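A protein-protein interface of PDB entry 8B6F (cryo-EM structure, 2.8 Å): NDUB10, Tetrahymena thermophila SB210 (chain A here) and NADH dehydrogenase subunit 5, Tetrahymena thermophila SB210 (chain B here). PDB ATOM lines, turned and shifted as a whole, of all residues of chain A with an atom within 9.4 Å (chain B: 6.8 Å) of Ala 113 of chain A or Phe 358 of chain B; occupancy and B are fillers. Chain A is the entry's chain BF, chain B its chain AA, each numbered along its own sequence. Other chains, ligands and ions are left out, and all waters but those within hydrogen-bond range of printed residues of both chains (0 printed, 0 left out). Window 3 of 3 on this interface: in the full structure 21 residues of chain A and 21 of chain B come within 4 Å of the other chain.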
ATOM      1  N   GLU A  64     -25.308  13.933  21.255  1.00  0.00           N
ATOM      2  CA  GLU A  64     -23.875  14.018  20.994  1.00  0.00           C
ATOM      3  C   GLU A  64     -23.161  12.784  21.530  1.00  0.00           C
ATOM      4  O   GLU A  64     -22.309  12.200  20.852  1.00  0.00           O
ATOM      5  CB  GLU A  64     -23.305  15.289  21.623  1.00  0.00           C
ATOM      6  CG  GLU A  64     -23.895  16.576  21.069  1.00  0.00           C
ATOM      7  CD  GLU A  64     -23.434  16.875  19.657  1.00  0.00           C
ATOM      8  OE1 GLU A  64     -22.822  15.990  19.025  1.00  0.00           O
ATOM      9  OE2 GLU A  64     -23.677  18.003  19.181  1.00  0.00           O
ATOM     10  N   ASN A  68     -21.098   9.867  19.402  1.00  0.00           N
ATOM     11  CA  ASN A  68     -19.799   9.379  19.852  1.00  0.00           C
ATOM     12  C   ASN A  68     -19.848   7.880  20.110  1.00  0.00           C
ATOM     13  O   ASN A  68     -18.870   7.167  19.864  1.00  0.00           O
ATOM     14  CB  ASN A  68     -19.353  10.125  21.109  1.00  0.00           C
ATOM     15  CG  ASN A  68     -18.961  11.558  20.828  1.00  0.00           C
ATOM     16  OD1 ASN A  68     -18.619  11.910  19.701  1.00  0.00           O
ATOM     17  ND2 ASN A  68     -18.999  12.393  21.857  1.00  0.00           N
ATOM     18  N   ARG A  71     -19.471   6.101  16.890  1.00  0.00           N
ATOM     19  CA  ARG A  71     -18.072   6.055  16.486  1.00  0.00           C
ATOM     20  C   ARG A  71     -17.310   4.998  17.276  1.00  0.00           C
ATOM     21  O   ARG A  71     -16.485   4.267  16.718  1.00  0.00           O
ATOM     22  CB  ARG A  71     -17.429   7.429  16.665  1.00  0.00           C
ATOM     23  CG  ARG A  71     -16.070   7.570  15.997  1.00  0.00           C
ATOM     24  CD  ARG A  71     -16.191   7.405  14.491  1.00  0.00           C
ATOM     25  NE  ARG A  71     -14.976   7.789  13.784  1.00  0.00           N
ATOM     26  CZ  ARG A  71     -13.990   6.962  13.469  1.00  0.00           C
ATOM     27  NH1 ARG A  71     -14.028   5.682  13.799  1.00  0.00           N
ATOM     28  NH2 ARG A  71     -12.938   7.430  12.805  1.00  0.00           N
ATOM     29  N   LYS A  72     -17.544   4.930  18.586  1.00  0.00           N
ATOM     30  CA  LYS A  72     -16.873   3.926  19.404  1.00  0.00           C
ATOM     31  C   LYS A  72     -17.263   2.518  18.975  1.00  0.00           C
ATOM     32  O   LYS A  72     -16.417   1.619  18.926  1.00  0.00           O
ATOM     33  CB  LYS A  72     -17.204   4.149  20.878  1.00  0.00           C
ATOM     34  CG  LYS A  72     -16.686   5.464  21.429  1.00  0.00           C
ATOM     35  CD  LYS A  72     -17.460   5.900  22.661  1.00  0.00           C
ATOM     36  CE  LYS A  72     -17.360   4.876  23.777  1.00  0.00           C
ATOM     37  NZ  LYS A  72     -18.101   5.316  24.990  1.00  0.00           N
ATOM     38  N   ASN A  75     -15.519   1.631  15.716  1.00  0.00           N
ATOM     39  CA  ASN A  75     -14.114   1.350  15.995  1.00  0.00           C
ATOM     40  C   ASN A  75     -13.944  -0.035  16.607  1.00  0.00           C
ATOM     41  O   ASN A  75     -13.020  -0.772  16.246  1.00  0.00           O
ATOM     42  CB  ASN A  75     -13.531   2.417  16.921  1.00  0.00           C
ATOM     43  CG  ASN A  75     -13.300   3.738  16.218  1.00  0.00           C
ATOM     44  OD1 ASN A  75     -12.846   3.773  15.076  1.00  0.00           O
ATOM     45  ND2 ASN A  75     -13.601   4.834  16.901  1.00  0.00           N
ATOM     46  N   LEU A 105     -18.691   8.954   9.983  1.00  0.00           N
ATOM     47  CA  LEU A 105     -18.694   9.320  11.394  1.00  0.00           C
ATOM     48  C   LEU A 105     -17.449  10.109  11.782  1.00  0.00           C
ATOM     49  O   LEU A 105     -16.949   9.968  12.901  1.00  0.00           O
ATOM     50  CB  LEU A 105     -18.823   8.070  12.263  1.00  0.00           C
ATOM     51  CG  LEU A 105     -20.093   7.241  12.077  1.00  0.00           C
ATOM     52  CD1 LEU A 105     -20.007   5.954  12.874  1.00  0.00           C
ATOM     53  CD2 LEU A 105     -21.324   8.033  12.484  1.00  0.00           C
ATOM     54  N   SER A 106     -16.935  10.935  10.875  1.00  0.00           N
ATOM     55  CA  SER A 106     -15.723  11.695  11.136  1.00  0.00           C
ATOM     56  C   SER A 106     -16.019  12.863  12.074  1.00  0.00           C
ATOM     57  O   SER A 106     -17.141  13.050  12.550  1.00  0.00           O
ATOM     58  CB  SER A 106     -15.116  12.185   9.825  1.00  0.00           C
ATOM     59  OG  SER A 106     -14.760  11.095   8.993  1.00  0.00           O
ATOM     60  N   SER A 107     -14.989  13.668  12.336  1.00  0.00           N
ATOM     61  CA  SER A 107     -15.108  14.717  13.344  1.00  0.00           C
ATOM     62  C   SER A 107     -16.246  15.691  13.073  1.00  0.00           C
ATOM     63  O   SER A 107     -16.950  16.051  14.034  1.00  0.00           O
ATOM     64  CB  SER A 107     -13.777  15.469  13.471  1.00  0.00           C
ATOM     65  OG  SER A 107     -13.540  16.304  12.354  1.00  0.00           O
ATOM     66  N   VAL A 110     -19.413  13.813  14.261  1.00  0.00           N
ATOM     67  CA  VAL A 110     -19.391  13.377  15.650  1.00  0.00           C
ATOM     68  C   VAL A 110     -18.277  14.129  16.364  1.00  0.00           C
ATOM     69  O   VAL A 110     -17.152  14.208  15.860  1.00  0.00           O
ATOM     70  CB  VAL A 110     -19.189  11.852  15.767  1.00  0.00           C
ATOM     71  CG1 VAL A 110     -20.158  11.123  14.852  1.00  0.00           C
ATOM     72  CG2 VAL A 110     -17.753  11.446  15.455  1.00  0.00           C
ATOM     73  N   ARG A 111     -18.593  14.694  17.526  1.00  0.00           N
ATOM     74  CA  ARG A 111     -17.623  15.444  18.322  1.00  0.00           C
ATOM     75  C   ARG A 111     -16.888  14.451  19.210  1.00  0.00           C
ATOM     76  O   ARG A 111     -17.314  14.146  20.324  1.00  0.00           O
ATOM     77  CB  ARG A 111     -18.323  16.526  19.130  1.00  0.00           C
ATOM     78  CG  ARG A 111     -17.424  17.309  20.078  1.00  0.00           C
ATOM     79  CD  ARG A 111     -18.183  17.718  21.327  1.00  0.00           C
ATOM     80  NE  ARG A 111     -18.604  16.560  22.105  1.00  0.00           N
ATOM     81  CZ  ARG A 111     -19.488  16.597  23.092  1.00  0.00           C
ATOM     82  NH1 ARG A 111     -20.082  17.724  23.447  1.00  0.00           N
ATOM     83  NH2 ARG A 111     -19.782  15.474  23.741  1.00  0.00           N
ATOM     84  N   GLY A 112     -15.768  13.940  18.714  1.00  0.00           N
ATOM     85  CA  GLY A 112     -15.009  12.967  19.471  1.00  0.00           C
ATOM     86  C   GLY A 112     -14.501  13.517  20.786  1.00  0.00           C
ATOM     87  O   GLY A 112     -14.982  13.131  21.854  1.00  0.00           O
ATOM     88  N   ALA A 113     -13.547  14.445  20.719  1.00  0.00           N
ATOM     89  CA  ALA A 113     -12.932  15.006  21.911  1.00  0.00           C
ATOM     90  C   ALA A 113     -12.875  16.524  21.885  1.00  0.00           C
ATOM     91  O   ALA A 113     -12.295  17.120  22.798  1.00  0.00           O
ATOM     92  CB  ALA A 113     -11.514  14.450  22.093  1.00  0.00           C
ATOM     93  N   HIS A 114     -13.455  17.160  20.875  1.00  0.00           N
ATOM     94  CA  HIS A 114     -13.436  18.609  20.784  1.00  0.00           C
ATOM     95  C   HIS A 114     -14.258  19.217  21.912  1.00  0.00           C
ATOM     96  O   HIS A 114     -15.234  18.632  22.386  1.00  0.00           O
ATOM     97  CB  HIS A 114     -13.981  19.061  19.431  1.00  0.00           C
ATOM     98  CG  HIS A 114     -13.359  18.355  18.268  1.00  0.00           C
ATOM     99  ND1 HIS A 114     -12.161  17.677  18.363  1.00  0.00           N
ATOM    100  CD2 HIS A 114     -13.772  18.208  16.989  1.00  0.00           C
ATOM    101  CE1 HIS A 114     -11.863  17.148  17.191  1.00  0.00           C
ATOM    102  NE2 HIS A 114     -12.823  17.456  16.339  1.00  0.00           N
ATOM    103  N   PHE A 115     -13.846  20.408  22.348  1.00  0.00           N
ATOM    104  CA  PHE A 115     -14.552  21.073  23.436  1.00  0.00           C
ATOM    105  C   PHE A 115     -16.012  21.309  23.080  1.00  0.00           C
ATOM    106  O   PHE A 115     -16.904  21.087  23.908  1.00  0.00           O
ATOM    107  CB  PHE A 115     -13.869  22.400  23.773  1.00  0.00           C
ATOM    108  CG  PHE A 115     -12.602  22.261  24.577  1.00  0.00           C
ATOM    109  CD1 PHE A 115     -12.468  21.276  25.544  1.00  0.00           C
ATOM    110  CD2 PHE A 115     -11.552  23.139  24.377  1.00  0.00           C
ATOM    111  CE1 PHE A 115     -11.307  21.163  26.284  1.00  0.00           C
ATOM    112  CE2 PHE A 115     -10.389  23.033  25.114  1.00  0.00           C
ATOM    113  CZ  PHE A 115     -10.266  22.044  26.070  1.00  0.00           C
ATOM    114  N   GLN A 116     -16.280  21.758  21.858  1.00  0.00           N
ATOM    115  CA  GLN A 116     -17.626  22.101  21.428  1.00  0.00           C
ATOM    116  C   GLN A 116     -17.892  21.524  20.048  1.00  0.00           C
ATOM    117  O   GLN A 116     -17.041  21.599  19.157  1.00  0.00           O
ATOM    118  CB  GLN A 116     -17.824  23.621  21.394  1.00  0.00           C
ATOM    119  CG  GLN A 116     -19.224  24.063  20.999  1.00  0.00           C
ATOM    120  CD  GLN A 116     -20.244  23.802  22.086  1.00  0.00           C
ATOM    121  OE1 GLN A 116     -20.624  24.711  22.822  1.00  0.00           O
ATOM    122  NE2 GLN A 116     -20.699  22.559  22.191  1.00  0.00           N
ATOM    123  N   ALA A 117     -19.078  20.947  19.880  1.00  0.00           N
ATOM    124  CA  ALA A 117     -19.579  20.551  18.570  1.00  0.00           C
ATOM    125  C   ALA A 117     -20.295  21.751  17.967  1.00  0.00           C
ATOM    126  O   ALA A 117     -21.397  22.103  18.396  1.00  0.00           O
ATOM    127  CB  ALA A 117     -20.521  19.357  18.688  1.00  0.00           C
ATOM    128  N   LEU B 238     -11.503   9.186  29.311  1.00  0.00           N
ATOM    129  CA  LEU B 238     -10.688  10.149  28.583  1.00  0.00           C
ATOM    130  C   LEU B 238     -11.517  11.120  27.752  1.00  0.00           C
ATOM    131  O   LEU B 238     -10.953  11.852  26.929  1.00  0.00           O
ATOM    132  CB  LEU B 238      -9.684   9.413  27.689  1.00  0.00           C
ATOM    133  CG  LEU B 238      -8.641   8.562  28.422  1.00  0.00           C
ATOM    134  CD1 LEU B 238      -7.772   7.816  27.429  1.00  0.00           C
ATOM    135  CD2 LEU B 238      -7.776   9.411  29.341  1.00  0.00           C
ATOM    136  N   SER B 239     -12.831  11.150  27.939  1.00  0.00           N
ATOM    137  CA  SER B 239     -13.693  12.115  27.267  1.00  0.00           C
ATOM    138  C   SER B 239     -15.040  12.115  27.979  1.00  0.00           C
ATOM    139  O   SER B 239     -15.222  11.445  28.999  1.00  0.00           O
ATOM    140  CB  SER B 239     -13.833  11.799  25.775  1.00  0.00           C
ATOM    141  OG  SER B 239     -12.576  11.834  25.126  1.00  0.00           O
ATOM    142  N   ASN B 240     -15.994  12.869  27.431  1.00  0.00           N
ATOM    143  CA  ASN B 240     -17.284  13.019  28.091  1.00  0.00           C
ATOM    144  C   ASN B 240     -17.978  11.676  28.275  1.00  0.00           C
ATOM    145  O   ASN B 240     -18.731  11.496  29.240  1.00  0.00           O
ATOM    146  CB  ASN B 240     -18.168  13.975  27.291  1.00  0.00           C
ATOM    147  CG  ASN B 240     -19.445  14.328  28.016  1.00  0.00           C
ATOM    148  OD1 ASN B 240     -19.587  14.067  29.209  1.00  0.00           O
ATOM    149  ND2 ASN B 240     -20.384  14.936  27.300  1.00  0.00           N
ATOM    150  N   PHE B 242     -16.153   8.579  26.938  1.00  0.00           N
ATOM    151  CA  PHE B 242     -15.162   7.601  26.521  1.00  0.00           C
ATOM    152  C   PHE B 242     -14.480   6.997  27.739  1.00  0.00           C
ATOM    153  O   PHE B 242     -14.397   7.620  28.800  1.00  0.00           O
ATOM    154  CB  PHE B 242     -14.118   8.245  25.606  1.00  0.00           C
ATOM    155  CG  PHE B 242     -13.205   7.263  24.938  1.00  0.00           C
ATOM    156  CD1 PHE B 242     -13.630   6.549  23.833  1.00  0.00           C
ATOM    157  CD2 PHE B 242     -11.916   7.067  25.401  1.00  0.00           C
ATOM    158  CE1 PHE B 242     -12.792   5.650  23.209  1.00  0.00           C
ATOM    159  CE2 PHE B 242     -11.071   6.170  24.781  1.00  0.00           C
ATOM    160  CZ  PHE B 242     -11.510   5.460  23.683  1.00  0.00           C
ATOM    161  N   ALA B 353       1.512  13.095  19.352  1.00  0.00           N
ATOM    162  CA  ALA B 353       1.077  12.216  18.271  1.00  0.00           C
ATOM    163  C   ALA B 353      -0.189  11.459  18.653  1.00  0.00           C
ATOM    164  O   ALA B 353      -1.111  11.324  17.841  1.00  0.00           O
ATOM    165  CB  ALA B 353       2.194  11.239  17.908  1.00  0.00           C
ATOM    166  N   ILE B 354      -0.248  10.954  19.886  1.00  0.00           N
ATOM    167  CA  ILE B 354      -1.433  10.235  20.343  1.00  0.00           C
ATOM    168  C   ILE B 354      -2.639  11.165  20.373  1.00  0.00           C
ATOM    169  O   ILE B 354      -3.757  10.765  20.027  1.00  0.00           O
ATOM    170  CB  ILE B 354      -1.169   9.598  21.721  1.00  0.00           C
ATOM    171  CG1 ILE B 354      -0.072   8.537  21.606  1.00  0.00           C
ATOM    172  CG2 ILE B 354      -2.444   8.981  22.281  1.00  0.00           C
ATOM    173  CD1 ILE B 354       0.495   8.091  22.936  1.00  0.00           C
ATOM    174  N   LEU B 355      -2.437  12.414  20.792  1.00  0.00           N
ATOM    175  CA  LEU B 355      -3.535  13.374  20.800  1.00  0.00           C
ATOM    176  C   LEU B 355      -4.043  13.640  19.389  1.00  0.00           C
ATOM    177  O   LEU B 355      -5.254  13.737  19.166  1.00  0.00           O
ATOM    178  CB  LEU B 355      -3.093  14.678  21.463  1.00  0.00           C
ATOM    179  CG  LEU B 355      -2.873  14.635  22.976  1.00  0.00           C
ATOM    180  CD1 LEU B 355      -2.291  15.951  23.440  1.00  0.00           C
ATOM    181  CD2 LEU B 355      -4.160  14.333  23.725  1.00  0.00           C
ATOM    182  N   ILE B 356      -3.132  13.771  18.422  1.00  0.00           N
ATOM    183  CA  ILE B 356      -3.553  13.962  17.037  1.00  0.00           C
ATOM    184  C   ILE B 356      -4.366  12.764  16.567  1.00  0.00           C
ATOM    185  O   ILE B 356      -5.410  12.917  15.924  1.00  0.00           O
ATOM    186  CB  ILE B 356      -2.329  14.204  16.134  1.00  0.00           C
ATOM    187  CG1 ILE B 356      -1.657  15.531  16.492  1.00  0.00           C
ATOM    188  CG2 ILE B 356      -2.737  14.208  14.665  1.00  0.00           C
ATOM    189  CD1 ILE B 356      -0.328  15.752  15.799  1.00  0.00           C
ATOM    190  N   ILE B 357      -3.900  11.555  16.875  1.00  0.00           N
ATOM    191  CA  ILE B 357      -4.617  10.355  16.459  1.00  0.00           C
ATOM    192  C   ILE B 357      -6.010  10.329  17.073  1.00  0.00           C
ATOM    193  O   ILE B 357      -6.998  10.023  16.394  1.00  0.00           O
ATOM    194  CB  ILE B 357      -3.806   9.101  16.832  1.00  0.00           C
ATOM    195  CG1 ILE B 357      -2.552   9.013  15.961  1.00  0.00           C
ATOM    196  CG2 ILE B 357      -4.653   7.840  16.686  1.00  0.00           C
ATOM    197  CD1 ILE B 357      -1.562   7.966  16.412  1.00  0.00           C
ATOM    198  N   PHE B 358      -6.114  10.651  18.363  1.00  0.00           N
ATOM    199  CA  PHE B 358      -7.415  10.629  19.025  1.00  0.00           C
ATOM    200  C   PHE B 358      -8.352  11.676  18.436  1.00  0.00           C
ATOM    201  O   PHE B 358      -9.545  11.416  18.247  1.00  0.00           O
ATOM    202  CB  PHE B 358      -7.232  10.846  20.527  1.00  0.00           C
ATOM    203  CG  PHE B 358      -8.456  10.538  21.338  1.00  0.00           C
ATOM    204  CD1 PHE B 358      -8.960   9.251  21.387  1.00  0.00           C
ATOM    205  CD2 PHE B 358      -9.085  11.527  22.074  1.00  0.00           C
ATOM    206  CE1 PHE B 358     -10.078   8.958  22.137  1.00  0.00           C
ATOM    207  CE2 PHE B 358     -10.205  11.239  22.828  1.00  0.00           C
ATOM    208  CZ  PHE B 358     -10.701   9.953  22.859  1.00  0.00           C
ATOM    209  N   SER B 359      -7.835  12.870  18.146  1.00  0.00           N
ATOM    210  CA  SER B 359      -8.672  13.904  17.546  1.00  0.00           C
ATOM    211  C   SER B 359      -9.178  13.481  16.173  1.00  0.00           C
ATOM    212  O   SER B 359     -10.342  13.721  15.832  1.00  0.00           O
ATOM    213  CB  SER B 359      -7.911  15.226  17.456  1.00  0.00           C
ATOM    214  OG  SER B 359      -7.618  15.721  18.752  1.00  0.00           O
ATOM    215  N   THR B 360      -8.318  12.856  15.370  1.00  0.00           N
ATOM    216  CA  THR B 360      -8.735  12.421  14.041  1.00  0.00           C
ATOM    217  C   THR B 360      -9.745  11.287  14.139  1.00  0.00           C
ATOM    218  O   THR B 360     -10.896  11.421  13.707  1.00  0.00           O
ATOM    219  CB  THR B 360      -7.515  11.977  13.235  1.00  0.00           C
ATOM    220  OG1 THR B 360      -6.530  13.018  13.242  1.00  0.00           O
ATOM    221  CG2 THR B 360      -7.911  11.659  11.802  1.00  0.00           C
ATOM    222  N   THR B 361      -9.332  10.161  14.713  1.00  0.00           N
ATOM    223  CA  THR B 361     -10.204   9.022  14.946  1.00  0.00           C
ATOM    224  C   THR B 361     -10.494   8.932  16.435  1.00  0.00           C
ATOM    225  O   THR B 361      -9.573   8.985  17.255  1.00  0.00           O
ATOM    226  CB  THR B 361      -9.562   7.721  14.457  1.00  0.00           C
ATOM    227  OG1 THR B 361      -8.458   7.380  15.305  1.00  0.00           O
ATOM    228  CG2 THR B 361      -9.064   7.874  13.032  1.00  0.00           C
ATOM    229  N   TYR B 362     -11.771   8.784  16.781  1.00  0.00           N
ATOM    230  CA  TYR B 362     -12.203   8.750  18.176  1.00  0.00           C
ATOM    231  C   TYR B 362     -11.926   7.371  18.778  1.00  0.00           C
ATOM    232  O   TYR B 362     -12.806   6.687  19.298  1.00  0.00           O
ATOM    233  CB  TYR B 362     -13.680   9.115  18.253  1.00  0.00           C
ATOM    234  CG  TYR B 362     -14.210   9.367  19.642  1.00  0.00           C
ATOM    235  CD1 TYR B 362     -13.548  10.210  20.523  1.00  0.00           C
ATOM    236  CD2 TYR B 362     -15.404   8.797  20.054  1.00  0.00           C
ATOM    237  CE1 TYR B 362     -14.047  10.451  21.786  1.00  0.00           C
ATOM    238  CE2 TYR B 362     -15.908   9.031  21.312  1.00  0.00           C
ATOM    239  CZ  TYR B 362     -15.227   9.859  22.174  1.00  0.00           C
ATOM    240  OH  TYR B 362     -15.736  10.097  23.426  1.00  0.00           O
ATOM    241  N   ASN B 363     -10.660   6.972  18.702  1.00  0.00           N
ATOM    242  CA  ASN B 363     -10.258   5.633  19.102  1.00  0.00           C
ATOM    243  C   ASN B 363      -8.769   5.620  19.400  1.00  0.00           C
ATOM    244  O   ASN B 363      -7.988   6.330  18.762  1.00  0.00           O
ATOM    245  CB  ASN B 363     -10.598   4.615  18.008  1.00  0.00           C
ATOM    246  CG  ASN B 363      -9.644   3.442  17.987  1.00  0.00           C
ATOM    247  OD1 ASN B 363      -9.836   2.457  18.698  1.00  0.00           O
ATOM    248  ND2 ASN B 363      -8.605   3.540  17.165  1.00  0.00           N
ATOM    249  N   LEU B 364      -8.388   4.799  20.380  1.00  0.00           N
ATOM    250  CA  LEU B 364      -6.993   4.627  20.767  1.00  0.00           C
ATOM    251  C   LEU B 364      -6.513   3.191  20.600  1.00  0.00           C
ATOM    252  O   LEU B 364      -5.379   2.880  20.983  1.00  0.00           O
ATOM    253  CB  LEU B 364      -6.791   5.080  22.217  1.00  0.00           C
ATOM    254  CG  LEU B 364      -7.068   6.562  22.480  1.00  0.00           C
ATOM    255  CD1 LEU B 364      -7.191   6.830  23.964  1.00  0.00           C
ATOM    256  CD2 LEU B 364      -5.977   7.428  21.877  1.00  0.00           C
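O of Tyr 362 of chain B is in hydrogen-bond range of ND2 of Asn 75 of chain A, 3.1 Å away.
The side-chain hydroxyl (OH) of Tyr 362 of chain B sits close to the backbone carbonyl oxygen (O) of Gly 112 of chain A.
O of Glu 64 of chain A lies close to ND2 of Asn 68 of chain A (3.5 Å).
The backbone carbonyl oxygen (O) of Leu 105 of chain A is in hydrogen-bond range of the guanidinium group (NE) of Arg 71 of chain A (3.1 Å).
The side-chain amide oxygen of Asn 75 of chain A sits at hydrogen-bond distance from the guanidinium group of Arg 71 of chain A (2.6 Å).
The side-chain amide oxygen (OD1) of Asn 68 of chain A sits close to the backbone carbonyl oxygen (O) of Arg 111 of chain A.
O of Leu 355 of chain B is in hydrogen-bond range of OG of Ser 359 of chain B.
The backbone carbonyl oxygen (O) of Ile 357 of chain B sits at hydrogen-bond distance from the side-chain hydroxyl (OG1) of Thr 361 of chain B, 3.2 Å away.
Among the printed residues, merely in contact across the chains: Asn 68 of chain A with Tyr 362 of chain B, Arg 71 of chain A with Thr 361 of chain B, Arg 71 of chain A with Tyr 362 of chain B, Lys 72 of chain A with Tyr 362 of chain B, Asn 75 of chain A with Asn 363 of chain B, Arg 111 of chain A with Asn 240 of chain B, Ala 113 of chain A with Phe 358 of chain B and His 114 of chain A with Ser 359 of chain B.
Ala 113 of chain A touches just one residue of chain B: Phe 358 (3.5 Å).
Phe 358 of chain B touches just one residue of chain A: Ala 113.
Of the printed residues of chain A, Ser 359 of chain B touches His 114 (3.99 Å).
Printed residues of chain B within 4 Å of Gly 112 of chain A: Tyr 362 (2.8 Å).
Ser 107 of chain A touches none of the printed residues of chain B.
The nearest printed residue of chain B that does not touch Lys 72 of chain A is Phe 242 of chain B (4.03 Å).
Of the 16 printed residues of chain A, 8 touch a printed residue of chain B.
Printed residues of chain A that touch a printed residue of chain B: Asn 68, Arg 71, Lys 72, Asn 75, Arg 111, Gly 112, Ala 113 and His 114.
Printed residues of chain B that touch a printed residue of chain A: Asn 240, Phe 358, Ser 359, Thr 361, Tyr 362 and Asn 363.
Hydrophobic or aromatic side chains of chain B within 4 Å of the printed part of chain A: Phe 358 and Tyr 362.
Among the printed residues, 10 pairs touch across the chains.
Among the printed residues, no Asp or Glu carboxylate lies within 4 Å of a Lys or Arg side-chain nitrogen of the other chain.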
